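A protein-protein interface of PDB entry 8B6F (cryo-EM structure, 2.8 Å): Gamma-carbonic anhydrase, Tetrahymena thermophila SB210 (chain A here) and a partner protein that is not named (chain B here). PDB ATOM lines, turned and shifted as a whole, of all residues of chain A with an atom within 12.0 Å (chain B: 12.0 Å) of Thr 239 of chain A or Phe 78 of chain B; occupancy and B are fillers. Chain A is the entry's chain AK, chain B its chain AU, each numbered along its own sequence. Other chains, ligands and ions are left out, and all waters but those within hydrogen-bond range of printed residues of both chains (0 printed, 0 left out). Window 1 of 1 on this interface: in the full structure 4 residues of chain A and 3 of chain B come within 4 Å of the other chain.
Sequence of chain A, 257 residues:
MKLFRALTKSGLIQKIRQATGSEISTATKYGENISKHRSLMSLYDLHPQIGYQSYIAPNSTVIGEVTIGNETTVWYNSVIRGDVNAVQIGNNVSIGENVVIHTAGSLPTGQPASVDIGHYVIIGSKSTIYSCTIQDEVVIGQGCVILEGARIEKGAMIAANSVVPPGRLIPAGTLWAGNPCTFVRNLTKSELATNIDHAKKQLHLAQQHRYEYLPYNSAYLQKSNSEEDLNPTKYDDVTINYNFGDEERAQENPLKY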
ATOM      1  N   LYS A 234      14.757  32.178 -27.116  1.00  0.00           N
ATOM      2  CA  LYS A 234      13.464  32.244 -26.453  1.00  0.00           C
ATOM      3  C   LYS A 234      13.537  31.488 -25.136  1.00  0.00           C
ATOM      4  O   LYS A 234      14.331  30.559 -24.979  1.00  0.00           O
ATOM      5  CB  LYS A 234      12.352  31.660 -27.331  1.00  0.00           C
ATOM      6  CG  LYS A 234      12.611  30.231 -27.783  1.00  0.00           C
ATOM      7  CD  LYS A 234      11.549  29.750 -28.762  1.00  0.00           C
ATOM      8  CE  LYS A 234      10.196  29.549 -28.093  1.00  0.00           C
ATOM      9  NZ  LYS A 234      10.231  28.488 -27.047  1.00  0.00           N
ATOM     10  N   TYR A 235      12.695  31.893 -24.192  1.00  0.00           N
ATOM     11  CA  TYR A 235      12.661  31.309 -22.861  1.00  0.00           C
ATOM     12  C   TYR A 235      11.335  30.600 -22.627  1.00  0.00           C
ATOM     13  O   TYR A 235      10.293  30.999 -23.154  1.00  0.00           O
ATOM     14  CB  TYR A 235      12.873  32.379 -21.786  1.00  0.00           C
ATOM     15  CG  TYR A 235      14.265  32.963 -21.781  1.00  0.00           C
ATOM     16  CD1 TYR A 235      14.619  33.974 -22.663  1.00  0.00           C
ATOM     17  CD2 TYR A 235      15.225  32.506 -20.889  1.00  0.00           C
ATOM     18  CE1 TYR A 235      15.892  34.510 -22.660  1.00  0.00           C
ATOM     19  CE2 TYR A 235      16.499  33.034 -20.878  1.00  0.00           C
ATOM     20  CZ  TYR A 235      16.826  34.037 -21.764  1.00  0.00           C
ATOM     21  OH  TYR A 235      18.096  34.564 -21.756  1.00  0.00           O
ATOM     22  N   ASP A 236      11.390  29.538 -21.829  1.00  0.00           N
ATOM     23  CA  ASP A 236      10.224  28.745 -21.474  1.00  0.00           C
ATOM     24  C   ASP A 236       9.916  28.908 -19.992  1.00  0.00           C
ATOM     25  O   ASP A 236      10.749  29.365 -19.206  1.00  0.00           O
ATOM     26  CB  ASP A 236      10.445  27.264 -21.794  1.00  0.00           C
ATOM     27  CG  ASP A 236      10.665  27.012 -23.272  1.00  0.00           C
ATOM     28  OD1 ASP A 236      10.044  27.716 -24.096  1.00  0.00           O
ATOM     29  OD2 ASP A 236      11.453  26.108 -23.612  1.00  0.00           O
ATOM     30  N   ASP A 237       8.697  28.531 -19.619  1.00  0.00           N
ATOM     31  CA  ASP A 237       8.267  28.579 -18.230  1.00  0.00           C
ATOM     32  C   ASP A 237       8.673  27.295 -17.518  1.00  0.00           C
ATOM     33  O   ASP A 237       8.518  26.196 -18.057  1.00  0.00           O
ATOM     34  CB  ASP A 237       6.753  28.777 -18.139  1.00  0.00           C
ATOM     35  CG  ASP A 237       6.286  29.048 -16.723  1.00  0.00           C
ATOM     36  OD1 ASP A 237       6.682  30.086 -16.155  1.00  0.00           O
ATOM     37  OD2 ASP A 237       5.522  28.226 -16.177  1.00  0.00           O
ATOM     38  N   VAL A 238       9.201  27.441 -16.306  1.00  0.00           N
ATOM     39  CA  VAL A 238       9.671  26.291 -15.538  1.00  0.00           C
ATOM     40  C   VAL A 238       8.457  25.468 -15.112  1.00  0.00           C
ATOM     41  O   VAL A 238       7.650  25.906 -14.288  1.00  0.00           O
ATOM     42  CB  VAL A 238      10.519  26.722 -14.334  1.00  0.00           C
ATOM     43  CG1 VAL A 238      11.761  27.459 -14.801  1.00  0.00           C
ATOM     44  CG2 VAL A 238       9.730  27.602 -13.366  1.00  0.00           C
ATOM     45  N   THR A 239       8.307  24.283 -15.703  1.00  0.00           N
ATOM     46  CA  THR A 239       7.232  23.363 -15.351  1.00  0.00           C
ATOM     47  C   THR A 239       7.724  22.241 -14.443  1.00  0.00           C
ATOM     48  O   THR A 239       7.271  22.115 -13.302  1.00  0.00           O
ATOM     49  CB  THR A 239       6.603  22.776 -16.622  1.00  0.00           C
ATOM     50  OG1 THR A 239       7.591  22.043 -17.359  1.00  0.00           O
ATOM     51  CG2 THR A 239       6.035  23.881 -17.497  1.00  0.00           C
ATOM     52  N   ILE A 240       8.653  21.426 -14.929  1.00  0.00           N
ATOM     53  CA  ILE A 240       9.200  20.324 -14.147  1.00  0.00           C
ATOM     54  C   ILE A 240      10.491  19.876 -14.814  1.00  0.00           C
ATOM     55  O   ILE A 240      10.602  19.868 -16.041  1.00  0.00           O
ATOM     56  CB  ILE A 240       8.181  19.165 -14.025  1.00  0.00           C
ATOM     57  CG1 ILE A 240       8.722  18.046 -13.129  1.00  0.00           C
ATOM     58  CG2 ILE A 240       7.841  18.600 -15.395  1.00  0.00           C
ATOM     59  CD1 ILE A 240       8.879  18.441 -11.684  1.00  0.00           C
ATOM     60  N   ASN A 241      11.465  19.497 -13.993  1.00  0.00           N
ATOM     61  CA  ASN A 241      12.723  18.959 -14.488  1.00  0.00           C
ATOM     62  C   ASN A 241      12.580  17.455 -14.657  1.00  0.00           C
ATOM     63  O   ASN A 241      12.137  16.761 -13.738  1.00  0.00           O
ATOM     64  CB  ASN A 241      13.869  19.277 -13.529  1.00  0.00           C
ATOM     65  CG  ASN A 241      14.229  20.745 -13.518  1.00  0.00           C
ATOM     66  OD1 ASN A 241      13.482  21.584 -14.019  1.00  0.00           O
ATOM     67  ND2 ASN A 241      15.378  21.065 -12.939  1.00  0.00           N
ATOM     68  N   TYR A 242      12.952  16.955 -15.835  1.00  0.00           N
ATOM     69  CA  TYR A 242      12.804  15.529 -16.094  1.00  0.00           C
ATOM     70  C   TYR A 242      13.546  14.695 -15.062  1.00  0.00           C
ATOM     71  O   TYR A 242      13.130  13.573 -14.756  1.00  0.00           O
ATOM     72  CB  TYR A 242      13.292  15.191 -17.503  1.00  0.00           C
ATOM     73  CG  TYR A 242      14.794  15.196 -17.647  1.00  0.00           C
ATOM     74  CD1 TYR A 242      15.496  16.384 -17.789  1.00  0.00           C
ATOM     75  CD2 TYR A 242      15.510  14.007 -17.647  1.00  0.00           C
ATOM     76  CE1 TYR A 242      16.869  16.387 -17.920  1.00  0.00           C
ATOM     77  CE2 TYR A 242      16.881  14.000 -17.778  1.00  0.00           C
ATOM     78  CZ  TYR A 242      17.555  15.192 -17.916  1.00  0.00           C
ATOM     79  OH  TYR A 242      18.922  15.186 -18.047  1.00  0.00           O
ATOM     80  N   ASN A 243      14.639  15.220 -14.519  1.00  0.00           N
ATOM     81  CA  ASN A 243      15.410  14.532 -13.486  1.00  0.00           C
ATOM     82  C   ASN A 243      15.001  15.026 -12.100  1.00  0.00           C
ATOM     83  O   ASN A 243      15.816  15.491 -11.305  1.00  0.00           O
ATOM     84  CB  ASN A 243      16.902  14.732 -13.726  1.00  0.00           C
ATOM     85  CG  ASN A 243      17.313  16.185 -13.643  1.00  0.00           C
ATOM     86  OD1 ASN A 243      16.517  17.083 -13.912  1.00  0.00           O
ATOM     87  ND2 ASN A 243      18.561  16.425 -13.265  1.00  0.00           N
ATOM     88  N   PHE A 244      13.707  14.919 -11.815  1.00  0.00           N
ATOM     89  CA  PHE A 244      13.167  15.296 -10.517  1.00  0.00           C
ATOM     90  C   PHE A 244      13.202  14.079  -9.603  1.00  0.00           C
ATOM     91  O   PHE A 244      12.657  13.025  -9.945  1.00  0.00           O
ATOM     92  CB  PHE A 244      11.741  15.831 -10.648  1.00  0.00           C
ATOM     93  CG  PHE A 244      11.174  16.368  -9.364  1.00  0.00           C
ATOM     94  CD1 PHE A 244      11.609  17.578  -8.852  1.00  0.00           C
ATOM     95  CD2 PHE A 244      10.198  15.666  -8.675  1.00  0.00           C
ATOM     96  CE1 PHE A 244      11.086  18.075  -7.671  1.00  0.00           C
ATOM     97  CE2 PHE A 244       9.671  16.157  -7.495  1.00  0.00           C
ATOM     98  CZ  PHE A 244      10.115  17.363  -6.992  1.00  0.00           C
ATOM     99  N   GLY A 245      13.842  14.226  -8.448  1.00  0.00           N
ATOM    100  CA  GLY A 245      14.062  13.102  -7.566  1.00  0.00           C
ATOM    101  C   GLY A 245      15.205  12.201  -7.967  1.00  0.00           C
ATOM    102  O   GLY A 245      15.339  11.110  -7.400  1.00  0.00           O
ATOM    103  N   VAL B  72      12.771  22.727   2.463  1.00  0.00           N
ATOM    104  CA  VAL B  72      11.348  22.544   2.191  1.00  0.00           C
ATOM    105  C   VAL B  72      11.021  22.985   0.769  1.00  0.00           C
ATOM    106  O   VAL B  72      10.276  22.310   0.049  1.00  0.00           O
ATOM    107  CB  VAL B  72      10.503  23.306   3.230  1.00  0.00           C
ATOM    108  CG1 VAL B  72       9.029  23.287   2.854  1.00  0.00           C
ATOM    109  CG2 VAL B  72      10.702  22.710   4.611  1.00  0.00           C
ATOM    110  N   LEU B  73      11.572  24.122   0.344  1.00  0.00           N
ATOM    111  CA  LEU B  73      11.273  24.654  -0.981  1.00  0.00           C
ATOM    112  C   LEU B  73      11.811  23.779  -2.104  1.00  0.00           C
ATOM    113  O   LEU B  73      11.281  23.834  -3.218  1.00  0.00           O
ATOM    114  CB  LEU B  73      11.849  26.062  -1.123  1.00  0.00           C
ATOM    115  CG  LEU B  73      10.822  27.188  -1.225  1.00  0.00           C
ATOM    116  CD1 LEU B  73      10.095  27.373   0.093  1.00  0.00           C
ATOM    117  CD2 LEU B  73      11.502  28.471  -1.661  1.00  0.00           C
ATOM    118  N   LYS B  74      12.850  22.984  -1.850  1.00  0.00           N
ATOM    119  CA  LYS B  74      13.446  22.182  -2.912  1.00  0.00           C
ATOM    120  C   LYS B  74      12.491  21.133  -3.464  1.00  0.00           C
ATOM    121  O   LYS B  74      12.776  20.557  -4.519  1.00  0.00           O
ATOM    122  CB  LYS B  74      14.720  21.507  -2.405  1.00  0.00           C
ATOM    123  CG  LYS B  74      15.930  22.423  -2.374  1.00  0.00           C
ATOM    124  CD  LYS B  74      17.107  21.761  -1.680  1.00  0.00           C
ATOM    125  CE  LYS B  74      18.278  22.721  -1.546  1.00  0.00           C
ATOM    126  NZ  LYS B  74      19.439  22.088  -0.862  1.00  0.00           N
ATOM    127  N   GLY B  75      11.380  20.866  -2.785  1.00  0.00           N
ATOM    128  CA  GLY B  75      10.401  19.919  -3.277  1.00  0.00           C
ATOM    129  C   GLY B  75       9.253  20.576  -4.015  1.00  0.00           C
ATOM    130  O   GLY B  75       8.186  19.975  -4.174  1.00  0.00           O
ATOM    131  N   LEU B  76       9.456  21.809  -4.471  1.00  0.00           N
ATOM    132  CA  LEU B  76       8.413  22.594  -5.115  1.00  0.00           C
ATOM    133  C   LEU B  76       8.579  22.559  -6.628  1.00  0.00           C
ATOM    134  O   LEU B  76       9.693  22.671  -7.145  1.00  0.00           O
ATOM    135  CB  LEU B  76       8.451  24.040  -4.616  1.00  0.00           C
ATOM    136  CG  LEU B  76       7.424  25.008  -5.203  1.00  0.00           C
ATOM    137  CD1 LEU B  76       6.008  24.522  -4.961  1.00  0.00           C
ATOM    138  CD2 LEU B  76       7.619  26.390  -4.611  1.00  0.00           C
ATOM    139  N   THR B  77       7.460  22.399  -7.333  1.00  0.00           N
ATOM    140  CA  THR B  77       7.448  22.362  -8.788  1.00  0.00           C
ATOM    141  C   THR B  77       6.221  23.106  -9.294  1.00  0.00           C
ATOM    142  O   THR B  77       5.261  23.335  -8.555  1.00  0.00           O
ATOM    143  CB  THR B  77       7.446  20.925  -9.326  1.00  0.00           C
ATOM    144  OG1 THR B  77       6.250  20.255  -8.912  1.00  0.00           O
ATOM    145  CG2 THR B  77       8.656  20.159  -8.813  1.00  0.00           C
ATOM    146  N   PHE B  78       6.263  23.487 -10.571  1.00  0.00           N
ATOM    147  CA  PHE B  78       5.154  24.194 -11.210  1.00  0.00           C
ATOM    148  C   PHE B  78       4.778  25.451 -10.430  1.00  0.00           C
ATOM    149  O   PHE B  78       3.601  25.771 -10.256  1.00  0.00           O
ATOM    150  CB  PHE B  78       3.936  23.281 -11.365  1.00  0.00           C
ATOM    151  CG  PHE B  78       4.067  22.268 -12.462  1.00  0.00           C
ATOM    152  CD1 PHE B  78       3.671  22.576 -13.752  1.00  0.00           C
ATOM    153  CD2 PHE B  78       4.566  21.006 -12.202  1.00  0.00           C
ATOM    154  CE1 PHE B  78       3.779  21.647 -14.763  1.00  0.00           C
ATOM    155  CE2 PHE B  78       4.678  20.071 -13.209  1.00  0.00           C
ATOM    156  CZ  PHE B  78       4.282  20.393 -14.493  1.00  0.00           C
ATOM    157  N   SER B  79       5.788  26.173  -9.958  1.00  0.00           N
ATOM    158  CA  SER B  79       5.587  27.354  -9.132  1.00  0.00           C
ATOM    159  C   SER B  79       6.213  28.567  -9.800  1.00  0.00           C
ATOM    160  O   SER B  79       7.289  28.474 -10.397  1.00  0.00           O
ATOM    161  CB  SER B  79       6.193  27.170  -7.741  1.00  0.00           C
ATOM    162  OG  SER B  79       7.601  27.066  -7.817  1.00  0.00           O
ATOM    163  N   SER B  80       5.529  29.701  -9.699  1.00  0.00           N
ATOM    164  CA  SER B  80       6.081  30.963 -10.153  1.00  0.00           C
ATOM    165  C   SER B  80       7.070  31.502  -9.121  1.00  0.00           C
ATOM    166  O   SER B  80       7.120  31.056  -7.973  1.00  0.00           O
ATOM    167  CB  SER B  80       4.965  31.975 -10.405  1.00  0.00           C
ATOM    168  OG  SER B  80       4.211  32.205  -9.228  1.00  0.00           O
ATOM    169  N   LEU B  81       7.869  32.480  -9.547  1.00  0.00           N
ATOM    170  CA  LEU B  81       8.851  33.068  -8.644  1.00  0.00           C
ATOM    171  C   LEU B  81       8.169  33.737  -7.458  1.00  0.00           C
ATOM    172  O   LEU B  81       8.653  33.653  -6.325  1.00  0.00           O
ATOM    173  CB  LEU B  81       9.726  34.073  -9.395  1.00  0.00           C
ATOM    174  CG  LEU B  81      10.850  34.727  -8.587  1.00  0.00           C
ATOM    175  CD1 LEU B  81      11.857  33.692  -8.117  1.00  0.00           C
ATOM    176  CD2 LEU B  81      11.541  35.803  -9.402  1.00  0.00           C
ATOM    177  N   ASN B  82       7.048  34.415  -7.701  1.00  0.00           N
ATOM    178  CA  ASN B  82       6.341  35.085  -6.616  1.00  0.00           C
ATOM    179  C   ASN B  82       5.849  34.081  -5.581  1.00  0.00           C
ATOM    180  O   ASN B  82       5.989  34.298  -4.373  1.00  0.00           O
ATOM    181  CB  ASN B  82       5.175  35.895  -7.178  1.00  0.00           C
ATOM    182  CG  ASN B  82       4.527  36.781  -6.137  1.00  0.00           C
ATOM    183  OD1 ASN B  82       5.161  37.170  -5.158  1.00  0.00           O
ATOM    184  ND2 ASN B  82       3.257  37.103  -6.341  1.00  0.00           N
ATOM    185  N   TYR B  83       5.255  32.976  -6.036  1.00  0.00           N
ATOM    186  CA  TYR B  83       4.765  31.974  -5.096  1.00  0.00           C
ATOM    187  C   TYR B  83       5.911  31.289  -4.365  1.00  0.00           C
ATOM    188  O   TYR B  83       5.795  30.976  -3.175  1.00  0.00           O
ATOM    189  CB  TYR B  83       3.906  30.938  -5.816  1.00  0.00           C
ATOM    190  CG  TYR B  83       3.412  29.852  -4.892  1.00  0.00           C
ATOM    191  CD1 TYR B  83       2.505  30.137  -3.881  1.00  0.00           C
ATOM    192  CD2 TYR B  83       3.854  28.546  -5.028  1.00  0.00           C
ATOM    193  CE1 TYR B  83       2.053  29.150  -3.032  1.00  0.00           C
ATOM    194  CE2 TYR B  83       3.407  27.551  -4.182  1.00  0.00           C
ATOM    195  CZ  TYR B  83       2.507  27.860  -3.186  1.00  0.00           C
ATOM    196  OH  TYR B  83       2.057  26.873  -2.343  1.00  0.00           O
ATOM    197  N   ARG B  84       7.023  31.036  -5.058  1.00  0.00           N
ATOM    198  CA  ARG B  84       8.171  30.424  -4.401  1.00  0.00           C
ATOM    199  C   ARG B  84       8.716  31.328  -3.304  1.00  0.00           C
ATOM    200  O   ARG B  84       9.025  30.865  -2.201  1.00  0.00           O
ATOM    201  CB  ARG B  84       9.257  30.114  -5.429  1.00  0.00           C
ATOM    202  CG  ARG B  84      10.459  29.382  -4.858  1.00  0.00           C
ATOM    203  CD  ARG B  84      11.503  29.126  -5.930  1.00  0.00           C
ATOM    204  NE  ARG B  84      10.987  28.289  -7.007  1.00  0.00           N
ATOM    205  CZ  ARG B  84      11.022  26.964  -7.016  1.00  0.00           C
ATOM    206  NH1 ARG B  84      11.539  26.277  -6.010  1.00  0.00           N
ATOM    207  NH2 ARG B  84      10.526  26.310  -8.062  1.00  0.00           N
ATOM    208  N   ARG B  85       8.854  32.623  -3.593  1.00  0.00           N
ATOM    209  CA  ARG B  85       9.338  33.557  -2.583  1.00  0.00           C
ATOM    210  C   ARG B  85       8.353  33.670  -1.427  1.00  0.00           C
ATOM    211  O   ARG B  85       8.756  33.750  -0.263  1.00  0.00           O
ATOM    212  CB  ARG B  85       9.599  34.921  -3.220  1.00  0.00           C
ATOM    213  CG  ARG B  85      10.731  34.887  -4.239  1.00  0.00           C
ATOM    214  CD  ARG B  85      10.786  36.136  -5.107  1.00  0.00           C
ATOM    215  NE  ARG B  85      11.409  37.270  -4.434  1.00  0.00           N
ATOM    216  CZ  ARG B  85      10.755  38.303  -3.917  1.00  0.00           C
ATOM    217  NH1 ARG B  85       9.434  38.383  -3.959  1.00  0.00           N
ATOM    218  NH2 ARG B  85      11.445  39.283  -3.344  1.00  0.00           N
ATOM    219  N   LEU B  87       6.278  31.310  -0.386  1.00  0.00           N
ATOM    220  CA  LEU B  87       6.378  30.085   0.399  1.00  0.00           C
ATOM    221  C   LEU B  87       7.622  30.096   1.275  1.00  0.00           C
ATOM    222  O   LEU B  87       7.574  29.681   2.439  1.00  0.00           O
ATOM    223  CB  LEU B  87       6.379  28.870  -0.527  1.00  0.00           C
ATOM    224  CG  LEU B  87       6.483  27.502   0.152  1.00  0.00           C
ATOM    225  CD1 LEU B  87       5.321  27.261   1.102  1.00  0.00           C
ATOM    226  CD2 LEU B  87       6.551  26.405  -0.892  1.00  0.00           C
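Lys 234 of chain A touches none of the printed residues of chain B. Asp 237 of chain A touches none of the printed residues of chain B. Printed residues of chain B within 4 Å of Val 238 of chain A: Ser 79. Ile 240 of chain A touches just these residues of chain B: Thr 77 (3.4 Å) and Phe 78 (3.7 Å). Printed residues of chain B within 4 Å of Phe 244 of chain A: Thr 77 (3.4 Å). Val 72 of chain B touches none of the printed residues of chain A. Leu 76 of chain B touches none of the printed residues of chain A. Of chain A, only Thr 239 and Ile 240 come within 4 Å of Phe 78 of chain B. No residue of chain A comes within 4 Å of Ser 80 of chain B. The nearest residue of chain B that does not touch Thr 239 of chain A is Thr 77 of chain B (4.2 Å). The nearest printed residue of chain B that does not touch Phe 244 of chain A is Gly 75 of chain B (4.3 Å).
N of Phe 78 of chain B sits close to O of Thr 239 of chain A (3.2 Å).
Among the printed residues, 5 pairs touch across the chains. Among the printed residues, no Asp or Glu carboxylate lies within 4 Å of a Lys or Arg side-chain nitrogen of the other chain.
Val 238 of chain A touches Ser 79 of chain B. CG2 of Thr 77 of chain B touches CD1 of Ile 240 of chain A, at 3.4 Å. Ile 240 of chain A touches Phe 78 of chain B. CE1 of Phe 244 of chain A touches CG2 of Thr 77 of chain B, 3.4 Å away.
OG of Ser 79 of chain B is in hydrogen-bond range of NH2 of Arg 84 of chain B.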
